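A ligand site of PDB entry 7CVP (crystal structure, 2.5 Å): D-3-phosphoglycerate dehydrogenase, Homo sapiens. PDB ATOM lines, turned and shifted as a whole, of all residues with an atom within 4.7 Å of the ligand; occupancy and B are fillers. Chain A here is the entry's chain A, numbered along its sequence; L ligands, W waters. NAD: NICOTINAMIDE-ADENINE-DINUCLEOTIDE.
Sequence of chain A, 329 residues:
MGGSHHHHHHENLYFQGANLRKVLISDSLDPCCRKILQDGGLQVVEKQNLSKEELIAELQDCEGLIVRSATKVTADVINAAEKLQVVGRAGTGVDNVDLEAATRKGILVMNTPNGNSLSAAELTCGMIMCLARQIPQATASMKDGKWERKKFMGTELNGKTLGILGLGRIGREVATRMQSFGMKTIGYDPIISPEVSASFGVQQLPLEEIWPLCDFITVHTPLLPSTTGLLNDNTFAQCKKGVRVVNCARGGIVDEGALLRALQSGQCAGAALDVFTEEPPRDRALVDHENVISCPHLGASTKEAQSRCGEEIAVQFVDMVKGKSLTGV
Water W1 lies within hydrogen-bond range of an oxygen (O4D) of the ligand (2.6 Å), a ring nitrogen (ND1) of His 220 (3.1 Å) and the backbone carbonyl oxygen (O) of Cys 248 (3.2 Å).
An oxygen (O3B) of the ligand is in hydrogen-bond range of the backbone NH (N) of Gly 168 (3.5 Å). N of Ile 170 is in hydrogen-bond range of O2N of the ligand, 2.9 Å away. The side-chain carboxylate of Asp 189 lies within hydrogen-bond range of an oxygen (O2B) of the ligand (2.4 Å). The backbone carbonyl oxygen (O) of Cys 248 lies within hydrogen-bond range of a nitrogen (N7N) of the ligand (2.6 Å). NH2 of Arg 250 sits at hydrogen-bond distance from O2D of the ligand (3.3 Å). The backbone carbonyl oxygen (O) of Thr 221 lies within hydrogen-bond range of an oxygen (O3D) of the ligand (2.6 Å). The backbone NH (N) of Arg 169 is in hydrogen-bond range of an oxygen (O2A) of the ligand (3.0 Å). The backbone NH (N) of Ala 300 is in hydrogen-bond range of an oxygen (O7N) of the ligand. The guanidinium group (NH1) of Arg 169 is in salt-bridge range of an oxygen (O2A) of the ligand (2.9 Å). The backbone NH (N) of Gly 299 sits close to an oxygen (O7N) of the ligand, at 3.4 Å. OD2 of Asp 274 lies within hydrogen-bond range of N7N of the ligand (3.2 Å). N of Gly 166 sits close to N3A of the ligand.
The side-chain carboxylate of Asp 274 lies within hydrogen-bond range of the backbone NH of Gly 299 (2.8 Å). The backbone carbonyl oxygen of Gly 299 is in hydrogen-bond range of the backbone NH of Ala 120 (3.0 Å). The side-chain carboxylate of Asp 189 sits at hydrogen-bond distance from the backbone NH of Leu 167, at 2.6 Å. N of His 220 sits at hydrogen-bond distance from O of Leu 165 (2.6 Å). The backbone NH (N) of Ile 191 is in hydrogen-bond range of the side-chain carboxylate (OD1) of Asp 189, at 3.2 Å. The side-chain carboxylate (OD1) of Asp 189 lies within hydrogen-bond range of the backbone NH (N) of Ile 192 (3.3 Å). The side-chain carboxylate of Asp 274 is in hydrogen-bond range of the backbone NH of Leu 298. The backbone NH (N) of Gly 166 lies within hydrogen-bond range of the backbone carbonyl oxygen (O) of Tyr 188, at 3.2 Å.
CG2 of Thr 92 touches C2D of the ligand, 3.7 Å away. Asn 116 touches the ligand (CB to C5N, 3.8 Å). Leu 167 touches the ligand (C to O3B, 3.9 Å). CE1 of Tyr 188 touches N1A of the ligand, 3.3 Å away. Pro 190 touches the ligand (CD to N3A, 3.2 Å). Ile 191 touches the ligand. Ile 192 touches the ligand (CG1 to O3B, 3.2 Å). O of His 220 touches C5D of the ligand, at 3.6 Å. CA of Pro 222 touches O3D of the ligand, at 3.2 Å. Thr 227 touches the ligand (CG2 to N6A, 3.2 Å). Ala 249 touches the ligand. His 297 touches the ligand. Hydrophobic or aromatic side chains within 4 Å of the ligand: Ile 170, Tyr 188, Pro 190, Ile 191, Ile 192, Pro 222, Ala 249, His 297 and Ala 300. 23 residues have an atom within 4 Å of the ligand: Thr 92, Asn 116, Gly 166, Leu 167, Gly 168, Arg 169, Ile 170, Tyr 188, Asp 189, Pro 190, Ile 191, Ile 192, His 220, Thr 221, Pro 222, Thr 227, Cys 248, Ala 249, Arg 250, Asp 274, His 297, Gly 299 and Ala 300. The nearest printed residue that does not touch the ligand is Ser 226 (4.02 Å).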
ATOM      1  N   THR A  92     -18.628   7.977 -23.614  1.00  0.00           N
ATOM      2  CA  THR A  92     -18.400   9.450 -23.623  1.00  0.00           C
ATOM      3  C   THR A  92     -17.547   9.838 -22.401  1.00  0.00           C
ATOM      4  O   THR A  92     -18.152  10.007 -21.319  1.00  0.00           O
ATOM      5  CB  THR A  92     -19.727  10.226 -23.674  1.00  0.00           C
ATOM      6  OG1 THR A  92     -20.350   9.977 -24.932  1.00  0.00           O
ATOM      7  CG2 THR A  92     -19.553  11.721 -23.523  1.00  0.00           C
ATOM      8  N   PRO A 113     -17.364   9.744 -28.558  1.00  0.00           N
ATOM      9  CA  PRO A 113     -18.330  10.730 -28.067  1.00  0.00           C
ATOM     10  C   PRO A 113     -19.757  10.569 -28.628  1.00  0.00           C
ATOM     11  O   PRO A 113     -20.678  10.771 -27.882  1.00  0.00           O
ATOM     12  CB  PRO A 113     -17.751  12.082 -28.514  1.00  0.00           C
ATOM     13  CG  PRO A 113     -16.781  11.742 -29.623  1.00  0.00           C
ATOM     14  CD  PRO A 113     -16.237  10.371 -29.253  1.00  0.00           C
ATOM     15  N   ASN A 116     -23.222   7.021 -27.787  1.00  0.00           N
ATOM     16  CA  ASN A 116     -24.272   6.877 -26.745  1.00  0.00           C
ATOM     17  C   ASN A 116     -25.267   8.046 -26.807  1.00  0.00           C
ATOM     18  O   ASN A 116     -26.113   8.127 -25.902  1.00  0.00           O
ATOM     19  CB  ASN A 116     -23.683   6.825 -25.327  1.00  0.00           C
ATOM     20  CG  ASN A 116     -22.606   5.780 -25.168  1.00  0.00           C
ATOM     21  OD1 ASN A 116     -21.585   6.033 -24.532  1.00  0.00           O
ATOM     22  ND2 ASN A 116     -22.806   4.604 -25.750  1.00  0.00           N
ATOM     23  N   SER A 117     -25.150   8.933 -27.799  1.00  0.00           N
ATOM     24  CA  SER A 117     -25.855  10.239 -27.842  1.00  0.00           C
ATOM     25  C   SER A 117     -27.371  10.037 -27.835  1.00  0.00           C
ATOM     26  O   SER A 117     -28.027  10.546 -26.914  1.00  0.00           O
ATOM     27  CB  SER A 117     -25.410  11.040 -29.039  1.00  0.00           C
ATOM     28  OG  SER A 117     -23.992  11.117 -29.073  1.00  0.00           O
ATOM     29  N   ALA A 120     -28.771   7.827 -24.645  1.00  0.00           N
ATOM     30  CA  ALA A 120     -28.834   8.689 -23.434  1.00  0.00           C
ATOM     31  C   ALA A 120     -30.006   9.682 -23.573  1.00  0.00           C
ATOM     32  O   ALA A 120     -30.660   9.962 -22.542  1.00  0.00           O
ATOM     33  CB  ALA A 120     -27.521   9.415 -23.241  1.00  0.00           C
ATOM     34  N   LEU A 165     -29.902  22.227 -20.168  1.00  0.00           N
ATOM     35  CA  LEU A 165     -28.561  22.761 -19.810  1.00  0.00           C
ATOM     36  C   LEU A 165     -27.497  21.941 -20.558  1.00  0.00           C
ATOM     37  O   LEU A 165     -27.510  20.709 -20.441  1.00  0.00           O
ATOM     38  CB  LEU A 165     -28.370  22.718 -18.291  1.00  0.00           C
ATOM     39  CG  LEU A 165     -29.540  23.239 -17.451  1.00  0.00           C
ATOM     40  CD1 LEU A 165     -29.120  23.441 -15.998  1.00  0.00           C
ATOM     41  CD2 LEU A 165     -30.097  24.548 -18.014  1.00  0.00           C
ATOM     42  N   GLY A 166     -26.639  22.646 -21.318  1.00  0.00           N
ATOM     43  CA  GLY A 166     -25.713  22.069 -22.308  1.00  0.00           C
ATOM     44  C   GLY A 166     -26.474  21.527 -23.490  1.00  0.00           C
ATOM     45  O   GLY A 166     -27.281  20.609 -23.286  1.00  0.00           O
ATOM     46  N   LEU A 167     -26.250  22.088 -24.682  1.00  0.00           N
ATOM     47  CA  LEU A 167     -26.991  21.727 -25.926  1.00  0.00           C
ATOM     48  C   LEU A 167     -26.006  21.126 -26.940  1.00  0.00           C
ATOM     49  O   LEU A 167     -26.081  21.493 -28.124  1.00  0.00           O
ATOM     50  CB  LEU A 167     -27.692  22.969 -26.504  1.00  0.00           C
ATOM     51  CG  LEU A 167     -28.321  23.914 -25.486  1.00  0.00           C
ATOM     52  CD1 LEU A 167     -28.962  25.111 -26.175  1.00  0.00           C
ATOM     53  CD2 LEU A 167     -29.336  23.197 -24.618  1.00  0.00           C
ATOM     54  N   GLY A 168     -25.124  20.226 -26.480  1.00  0.00           N
ATOM     55  CA  GLY A 168     -24.235  19.450 -27.363  1.00  0.00           C
ATOM     56  C   GLY A 168     -25.014  18.435 -28.177  1.00  0.00           C
ATOM     57  O   GLY A 168     -26.076  18.789 -28.717  1.00  0.00           O
ATOM     58  N   ARG A 169     -24.521  17.197 -28.220  1.00  0.00           N
ATOM     59  CA  ARG A 169     -25.064  16.091 -29.041  1.00  0.00           C
ATOM     60  C   ARG A 169     -26.484  15.723 -28.557  1.00  0.00           C
ATOM     61  O   ARG A 169     -27.376  15.613 -29.416  1.00  0.00           O
ATOM     62  CB  ARG A 169     -24.111  14.887 -28.974  1.00  0.00           C
ATOM     63  CG  ARG A 169     -22.752  15.153 -29.619  1.00  0.00           C
ATOM     64  CD  ARG A 169     -21.692  14.152 -29.193  1.00  0.00           C
ATOM     65  NE  ARG A 169     -20.515  14.228 -30.044  1.00  0.00           N
ATOM     66  CZ  ARG A 169     -19.508  15.098 -29.910  1.00  0.00           C
ATOM     67  NH1 ARG A 169     -19.523  16.002 -28.941  1.00  0.00           N
ATOM     68  NH2 ARG A 169     -18.490  15.071 -30.755  1.00  0.00           N
ATOM     69  N   ILE A 170     -26.689  15.591 -27.239  1.00  0.00           N
ATOM     70  CA  ILE A 170     -27.916  14.993 -26.623  1.00  0.00           C
ATOM     71  C   ILE A 170     -28.980  16.093 -26.434  1.00  0.00           C
ATOM     72  O   ILE A 170     -30.177  15.810 -26.665  1.00  0.00           O
ATOM     73  CB  ILE A 170     -27.559  14.283 -25.301  1.00  0.00           C
ATOM     74  CG1 ILE A 170     -26.542  13.154 -25.528  1.00  0.00           C
ATOM     75  CG2 ILE A 170     -28.809  13.792 -24.574  1.00  0.00           C
ATOM     76  CD1 ILE A 170     -25.904  12.628 -24.261  1.00  0.00           C
ATOM     77  N   GLY A 171     -28.567  17.298 -26.018  1.00  0.00           N
ATOM     78  CA  GLY A 171     -29.480  18.443 -25.806  1.00  0.00           C
ATOM     79  C   GLY A 171     -30.454  18.642 -26.954  1.00  0.00           C
ATOM     80  O   GLY A 171     -31.671  18.732 -26.695  1.00  0.00           O
ATOM     81  N   TYR A 188     -29.595  26.947 -22.484  1.00  0.00           N
ATOM     82  CA  TYR A 188     -28.383  27.747 -22.173  1.00  0.00           C
ATOM     83  C   TYR A 188     -27.124  26.888 -22.353  1.00  0.00           C
ATOM     84  O   TYR A 188     -27.121  25.693 -21.984  1.00  0.00           O
ATOM     85  CB  TYR A 188     -28.470  28.339 -20.763  1.00  0.00           C
ATOM     86  CG  TYR A 188     -27.176  28.904 -20.252  1.00  0.00           C
ATOM     87  CD1 TYR A 188     -26.203  28.075 -19.715  1.00  0.00           C
ATOM     88  CD2 TYR A 188     -26.905  30.266 -20.336  1.00  0.00           C
ATOM     89  CE1 TYR A 188     -24.993  28.581 -19.256  1.00  0.00           C
ATOM     90  CE2 TYR A 188     -25.697  30.785 -19.875  1.00  0.00           C
ATOM     91  CZ  TYR A 188     -24.737  29.940 -19.335  1.00  0.00           C
ATOM     92  OH  TYR A 188     -23.546  30.422 -18.885  1.00  0.00           O
ATOM     93  N   ASP A 189     -26.067  27.506 -22.877  1.00  0.00           N
ATOM     94  CA  ASP A 189     -24.805  26.856 -23.295  1.00  0.00           C
ATOM     95  C   ASP A 189     -23.759  27.920 -23.572  1.00  0.00           C
ATOM     96  O   ASP A 189     -23.989  28.823 -24.377  1.00  0.00           O
ATOM     97  CB  ASP A 189     -25.050  25.963 -24.518  1.00  0.00           C
ATOM     98  CG  ASP A 189     -23.951  24.950 -24.766  1.00  0.00           C
ATOM     99  OD1 ASP A 189     -22.784  25.343 -24.726  1.00  0.00           O
ATOM    100  OD2 ASP A 189     -24.300  23.773 -25.005  1.00  0.00           O
ATOM    101  N   PRO A 190     -22.570  27.874 -22.919  1.00  0.00           N
ATOM    102  CA  PRO A 190     -21.566  28.911 -23.075  1.00  0.00           C
ATOM    103  C   PRO A 190     -20.852  28.937 -24.437  1.00  0.00           C
ATOM    104  O   PRO A 190     -20.420  30.016 -24.806  1.00  0.00           O
ATOM    105  CB  PRO A 190     -20.571  28.609 -21.943  1.00  0.00           C
ATOM    106  CG  PRO A 190     -20.681  27.119 -21.755  1.00  0.00           C
ATOM    107  CD  PRO A 190     -22.146  26.822 -21.987  1.00  0.00           C
ATOM    108  N   ILE A 191     -20.767  27.802 -25.156  1.00  0.00           N
ATOM    109  CA  ILE A 191     -20.057  27.731 -26.465  1.00  0.00           C
ATOM    110  C   ILE A 191     -21.079  27.712 -27.607  1.00  0.00           C
ATOM    111  O   ILE A 191     -20.968  28.601 -28.484  1.00  0.00           O
ATOM    112  CB  ILE A 191     -19.042  26.561 -26.545  1.00  0.00           C
ATOM    113  CG1 ILE A 191     -19.644  25.231 -27.008  1.00  0.00           C
ATOM    114  CG2 ILE A 191     -18.300  26.422 -25.216  1.00  0.00           C
ATOM    115  CD1 ILE A 191     -18.631  24.130 -27.230  1.00  0.00           C
ATOM    116  N   ILE A 192     -22.055  26.794 -27.608  1.00  0.00           N
ATOM    117  CA  ILE A 192     -23.080  26.665 -28.700  1.00  0.00           C
ATOM    118  C   ILE A 192     -23.824  27.995 -28.830  1.00  0.00           C
ATOM    119  O   ILE A 192     -24.361  28.481 -27.814  1.00  0.00           O
ATOM    120  CB  ILE A 192     -24.067  25.512 -28.449  1.00  0.00           C
ATOM    121  CG1 ILE A 192     -23.373  24.154 -28.284  1.00  0.00           C
ATOM    122  CG2 ILE A 192     -25.117  25.493 -29.566  1.00  0.00           C
ATOM    123  CD1 ILE A 192     -22.671  23.665 -29.525  1.00  0.00           C
ATOM    124  N   HIS A 220     -27.469  18.212 -19.811  1.00  0.00           N
ATOM    125  CA  HIS A 220     -26.637  17.502 -20.819  1.00  0.00           C
ATOM    126  C   HIS A 220     -25.354  18.306 -21.045  1.00  0.00           C
ATOM    127  O   HIS A 220     -25.051  18.648 -22.213  1.00  0.00           O
ATOM    128  CB  HIS A 220     -27.452  17.253 -22.098  1.00  0.00           C
ATOM    129  CG  HIS A 220     -28.797  16.677 -21.817  1.00  0.00           C
ATOM    130  ND1 HIS A 220     -28.964  15.331 -21.539  1.00  0.00           N
ATOM    131  CD2 HIS A 220     -30.008  17.259 -21.674  1.00  0.00           C
ATOM    132  CE1 HIS A 220     -30.242  15.107 -21.274  1.00  0.00           C
ATOM    133  NE2 HIS A 220     -30.899  16.279 -21.345  1.00  0.00           N
ATOM    134  N   THR A 221     -24.663  18.613 -19.938  1.00  0.00           N
ATOM    135  CA  THR A 221     -23.324  19.235 -19.876  1.00  0.00           C
ATOM    136  C   THR A 221     -22.309  18.181 -19.429  1.00  0.00           C
ATOM    137  O   THR A 221     -22.667  17.247 -18.720  1.00  0.00           O
ATOM    138  CB  THR A 221     -23.301  20.426 -18.901  1.00  0.00           C
ATOM    139  OG1 THR A 221     -23.326  19.929 -17.557  1.00  0.00           O
ATOM    140  CG2 THR A 221     -24.479  21.360 -19.085  1.00  0.00           C
ATOM    141  N   PRO A 222     -21.021  18.315 -19.793  1.00  0.00           N
ATOM    142  CA  PRO A 222     -19.968  17.510 -19.171  1.00  0.00           C
ATOM    143  C   PRO A 222     -19.850  17.914 -17.691  1.00  0.00           C
ATOM    144  O   PRO A 222     -20.454  18.896 -17.308  1.00  0.00           O
ATOM    145  CB  PRO A 222     -18.717  17.821 -19.988  1.00  0.00           C
ATOM    146  CG  PRO A 222     -18.989  19.195 -20.578  1.00  0.00           C
ATOM    147  CD  PRO A 222     -20.481  19.229 -20.821  1.00  0.00           C
ATOM    148  N   LEU A 223     -19.087  17.143 -16.908  1.00  0.00           N
ATOM    149  CA  LEU A 223     -18.824  17.422 -15.474  1.00  0.00           C
ATOM    150  C   LEU A 223     -17.552  18.267 -15.369  1.00  0.00           C
ATOM    151  O   LEU A 223     -16.460  17.720 -15.636  1.00  0.00           O
ATOM    152  CB  LEU A 223     -18.692  16.112 -14.692  1.00  0.00           C
ATOM    153  CG  LEU A 223     -18.568  16.255 -13.171  1.00  0.00           C
ATOM    154  CD1 LEU A 223     -19.723  17.048 -12.584  1.00  0.00           C
ATOM    155  CD2 LEU A 223     -18.476  14.888 -12.504  1.00  0.00           C
ATOM    156  N   LEU A 224     -17.706  19.546 -15.023  1.00  0.00           N
ATOM    157  CA  LEU A 224     -16.622  20.533 -14.795  1.00  0.00           C
ATOM    158  C   LEU A 224     -16.875  21.201 -13.448  1.00  0.00           C
ATOM    159  O   LEU A 224     -17.902  20.961 -12.828  1.00  0.00           O
ATOM    160  CB  LEU A 224     -16.634  21.553 -15.934  1.00  0.00           C
ATOM    161  CG  LEU A 224     -16.461  20.973 -17.344  1.00  0.00           C
ATOM    162  CD1 LEU A 224     -16.755  22.033 -18.392  1.00  0.00           C
ATOM    163  CD2 LEU A 224     -15.076  20.394 -17.542  1.00  0.00           C
ATOM    164  N   SER A 226     -17.549  24.314 -13.170  1.00  0.00           N
ATOM    165  CA  SER A 226     -18.581  25.319 -13.558  1.00  0.00           C
ATOM    166  C   SER A 226     -19.961  24.676 -13.655  1.00  0.00           C
ATOM    167  O   SER A 226     -20.952  25.425 -13.636  1.00  0.00           O
ATOM    168  CB  SER A 226     -18.207  26.011 -14.846  1.00  0.00           C
ATOM    169  OG  SER A 226     -18.301  25.122 -15.941  1.00  0.00           O
ATOM    170  N   THR A 227     -20.025  23.333 -13.770  1.00  0.00           N
ATOM    171  CA  THR A 227     -21.293  22.560 -13.827  1.00  0.00           C
ATOM    172  C   THR A 227     -21.494  21.765 -12.522  1.00  0.00           C
ATOM    173  O   THR A 227     -22.668  21.533 -12.173  1.00  0.00           O
ATOM    174  CB  THR A 227     -21.344  21.699 -15.084  1.00  0.00           C
ATOM    175  OG1 THR A 227     -20.127  20.951 -15.188  1.00  0.00           O
ATOM    176  CG2 THR A 227     -21.553  22.516 -16.331  1.00  0.00           C
ATOM    177  N   LEU A 230     -24.498  22.778 -10.681  1.00  0.00           N
ATOM    178  CA  LEU A 230     -25.243  23.671 -11.613  1.00  0.00           C
ATOM    179  C   LEU A 230     -26.653  23.908 -11.063  1.00  0.00           C
ATOM    180  O   LEU A 230     -27.102  25.067 -11.111  1.00  0.00           O
ATOM    181  CB  LEU A 230     -25.287  23.061 -13.015  1.00  0.00           C
ATOM    182  CG  LEU A 230     -25.636  24.015 -14.160  1.00  0.00           C
ATOM    183  CD1 LEU A 230     -24.651  25.176 -14.253  1.00  0.00           C
ATOM    184  CD2 LEU A 230     -25.688  23.259 -15.479  1.00  0.00           C
ATOM    185  N   CYS A 248     -29.351  12.809 -16.503  1.00  0.00           N
ATOM    186  CA  CYS A 248     -28.930  11.623 -17.294  1.00  0.00           C
ATOM    187  C   CYS A 248     -27.515  11.834 -17.875  1.00  0.00           C
ATOM    188  O   CYS A 248     -27.203  11.196 -18.900  1.00  0.00           O
ATOM    189  CB  CYS A 248     -29.946  11.328 -18.387  1.00  0.00           C
ATOM    190  SG  CYS A 248     -31.326  10.302 -17.800  1.00  0.00           S
ATOM    191  N   ALA A 249     -26.692  12.641 -17.200  1.00  0.00           N
ATOM    192  CA  ALA A 249     -25.391  13.147 -17.693  1.00  0.00           C
ATOM    193  C   ALA A 249     -24.246  12.665 -16.784  1.00  0.00           C
ATOM    194  O   ALA A 249     -23.652  11.612 -17.101  1.00  0.00           O
ATOM    195  CB  ALA A 249     -25.449  14.658 -17.799  1.00  0.00           C
ATOM    196  N   ARG A 250     -23.922  13.392 -15.704  1.00  0.00           N
ATOM    197  CA  ARG A 250     -22.897  12.974 -14.715  1.00  0.00           C
ATOM    198  C   ARG A 250     -23.415  13.211 -13.297  1.00  0.00           C
ATOM    199  O   ARG A 250     -24.250  14.117 -13.106  1.00  0.00           O
ATOM    200  CB  ARG A 250     -21.574  13.734 -14.910  1.00  0.00           C
ATOM    201  CG  ARG A 250     -20.628  13.071 -15.892  1.00  0.00           C
ATOM    202  CD  ARG A 250     -20.056  11.726 -15.438  1.00  0.00           C
ATOM    203  NE  ARG A 250     -19.431  11.038 -16.560  1.00  0.00           N
ATOM    204  CZ  ARG A 250     -20.084  10.344 -17.498  1.00  0.00           C
ATOM    205  NH1 ARG A 250     -21.405  10.213 -17.455  1.00  0.00           N
ATOM    206  NH2 ARG A 250     -19.409   9.776 -18.480  1.00  0.00           N
ATOM    207  N   ASP A 274     -30.216   8.937 -13.341  1.00  0.00           N
ATOM    208  CA  ASP A 274     -29.456   7.800 -13.920  1.00  0.00           C
ATOM    209  C   ASP A 274     -28.062   7.767 -13.270  1.00  0.00           C
ATOM    210  O   ASP A 274     -27.385   6.719 -13.389  1.00  0.00           O
ATOM    211  CB  ASP A 274     -29.391   7.985 -15.435  1.00  0.00           C
ATOM    212  CG  ASP A 274     -29.016   6.727 -16.188  1.00  0.00           C
ATOM    213  OD1 ASP A 274     -29.588   5.662 -15.878  1.00  0.00           O
ATOM    214  OD2 ASP A 274     -28.156   6.822 -17.095  1.00  0.00           O
ATOM    215  N   VAL A 275     -27.667   8.857 -12.590  1.00  0.00           N
ATOM    216  CA  VAL A 275     -26.260   9.155 -12.203  1.00  0.00           C
ATOM    217  C   VAL A 275     -26.218   9.764 -10.792  1.00  0.00           C
ATOM    218  O   VAL A 275     -27.161  10.516 -10.428  1.00  0.00           O
ATOM    219  CB  VAL A 275     -25.562  10.092 -13.201  1.00  0.00           C
ATOM    220  CG1 VAL A 275     -25.371   9.426 -14.562  1.00  0.00           C
ATOM    221  CG2 VAL A 275     -26.284  11.415 -13.359  1.00  0.00           C
ATOM    222  N   HIS A 297     -27.335   3.913 -13.983  1.00  0.00           N
ATOM    223  CA  HIS A 297     -26.467   4.531 -15.020  1.00  0.00           C
ATOM    224  C   HIS A 297     -26.658   3.778 -16.338  1.00  0.00           C
ATOM    225  O   HIS A 297     -25.661   3.225 -16.847  1.00  0.00           O
ATOM    226  CB  HIS A 297     -25.011   4.564 -14.531  1.00  0.00           C
ATOM    227  CG  HIS A 297     -24.181   5.623 -15.181  1.00  0.00           C
ATOM    228  ND1 HIS A 297     -23.401   6.507 -14.447  1.00  0.00           N
ATOM    229  CD2 HIS A 297     -24.022   5.955 -16.478  1.00  0.00           C
ATOM    230  CE1 HIS A 297     -22.783   7.324 -15.279  1.00  0.00           C
ATOM    231  NE2 HIS A 297     -23.139   7.008 -16.532  1.00  0.00           N
ATOM    232  N   LEU A 298     -27.888   3.767 -16.865  1.00  0.00           N
ATOM    233  CA  LEU A 298     -28.329   2.953 -18.032  1.00  0.00           C
ATOM    234  C   LEU A 298     -28.336   3.779 -19.336  1.00  0.00           C
ATOM    235  O   LEU A 298     -28.565   3.156 -20.395  1.00  0.00           O
ATOM    236  CB  LEU A 298     -29.718   2.372 -17.752  1.00  0.00           C
ATOM    237  CG  LEU A 298     -29.776   1.327 -16.644  1.00  0.00           C
ATOM    238  CD1 LEU A 298     -31.206   0.883 -16.397  1.00  0.00           C
ATOM    239  CD2 LEU A 298     -28.886   0.131 -16.955  1.00  0.00           C
ATOM    240  N   GLY A 299     -28.052   5.087 -19.272  1.00  0.00           N
ATOM    241  CA  GLY A 299     -28.069   5.988 -20.438  1.00  0.00           C
ATOM    242  C   GLY A 299     -27.379   5.407 -21.659  1.00  0.00           C
ATOM    243  O   GLY A 299     -27.834   5.707 -22.786  1.00  0.00           O
ATOM    244  N   ALA A 300     -26.327   4.604 -21.455  1.00  0.00           N
ATOM    245  CA  ALA A 300     -25.471   4.015 -22.515  1.00  0.00           C
ATOM    246  C   ALA A 300     -25.617   2.482 -22.553  1.00  0.00           C
ATOM    247  O   ALA A 300     -24.687   1.829 -23.077  1.00  0.00           O
ATOM    248  CB  ALA A 300     -24.035   4.403 -22.282  1.00  0.00           C
HETATM  249  PA  NAD L   1     -21.315  17.259 -25.828  1.00  0.00           P
HETATM  250  O1A NAD L   1     -19.867  17.273 -25.481  1.00  0.00           O
HETATM  251  O2A NAD L   1     -21.723  16.948 -27.228  1.00  0.00           O
HETATM  252  O5B NAD L   1     -21.999  18.639 -25.381  1.00  0.00           O
HETATM  253  C5B NAD L   1     -21.683  19.273 -24.112  1.00  0.00           C
HETATM  254  C4B NAD L   1     -22.311  20.644 -24.103  1.00  0.00           C
HETATM  255  O4B NAD L   1     -22.384  21.169 -22.755  1.00  0.00           O
HETATM  256  C3B NAD L   1     -21.563  21.702 -24.929  1.00  0.00           C
HETATM  257  O3B NAD L   1     -22.465  22.357 -25.820  1.00  0.00           O
HETATM  258  C2B NAD L   1     -21.019  22.653 -23.846  1.00  0.00           C
HETATM  259  O2B NAD L   1     -20.846  23.980 -24.295  1.00  0.00           O
HETATM  260  C1B NAD L   1     -22.146  22.555 -22.832  1.00  0.00           C
HETATM  261  N9A NAD L   1     -21.842  23.114 -21.519  1.00  0.00           N
HETATM  262  C8A NAD L   1     -20.690  22.963 -20.792  1.00  0.00           C
HETATM  263  N7A NAD L   1     -20.715  23.596 -19.651  1.00  0.00           N
HETATM  264  C5A NAD L   1     -21.955  24.214 -19.611  1.00  0.00           C
HETATM  265  C6A NAD L   1     -22.580  25.034 -18.660  1.00  0.00           C
HETATM  266  N6A NAD L   1     -22.022  25.402 -17.508  1.00  0.00           N
HETATM  267  N1A NAD L   1     -23.831  25.475 -18.932  1.00  0.00           N
HETATM  268  C2A NAD L   1     -24.395  25.099 -20.087  1.00  0.00           C
HETATM  269  N3A NAD L   1     -23.901  24.340 -21.065  1.00  0.00           N
HETATM  270  C4A NAD L   1     -22.659  23.921 -20.760  1.00  0.00           C
HETATM  271  O3  NAD L   1     -22.028  16.208 -24.847  1.00  0.00           O
HETATM  272  PN  NAD L   1     -23.142  15.075 -25.049  1.00  0.00           P
HETATM  273  O1N NAD L   1     -22.623  14.059 -26.033  1.00  0.00           O
HETATM  274  O2N NAD L   1     -24.451  15.729 -25.341  1.00  0.00           O
HETATM  275  O5D NAD L   1     -23.145  14.456 -23.568  1.00  0.00           O
HETATM  276  C5D NAD L   1     -23.501  15.376 -22.495  1.00  0.00           C
HETATM  277  C4D NAD L   1     -23.358  14.706 -21.149  1.00  0.00           C
HETATM  278  O4D NAD L   1     -24.029  13.417 -21.159  1.00  0.00           O
HETATM  279  C3D NAD L   1     -21.927  14.420 -20.680  1.00  0.00           C
HETATM  280  O3D NAD L   1     -21.786  14.828 -19.330  1.00  0.00           O
HETATM  281  C2D NAD L   1     -21.816  12.907 -20.886  1.00  0.00           C
HETATM  282  O2D NAD L   1     -20.858  12.252 -20.076  1.00  0.00           O
HETATM  283  C1D NAD L   1     -23.220  12.490 -20.481  1.00  0.00           C
HETATM  284  N1N NAD L   1     -23.582  11.094 -20.883  1.00  0.00           N
HETATM  285  C2N NAD L   1     -24.120  10.240 -19.947  1.00  0.00           C
HETATM  286  C3N NAD L   1     -24.392   8.928 -20.302  1.00  0.00           C
HETATM  287  C7N NAD L   1     -25.325   8.121 -19.434  1.00  0.00           C
HETATM  288  O7N NAD L   1     -25.179   6.907 -19.382  1.00  0.00           O
HETATM  289  N7N NAD L   1     -26.284   8.777 -18.790  1.00  0.00           N
HETATM  290  C4N NAD L   1     -23.803   8.415 -21.459  1.00  0.00           C
HETATM  291  C5N NAD L   1     -23.371   9.296 -22.423  1.00  0.00           C
HETATM  292  C6N NAD L   1     -23.374  10.646 -22.153  1.00  0.00           C
HETATM  293  O   HOH W   1     -26.620  13.346 -21.261  1.00  0.00           O
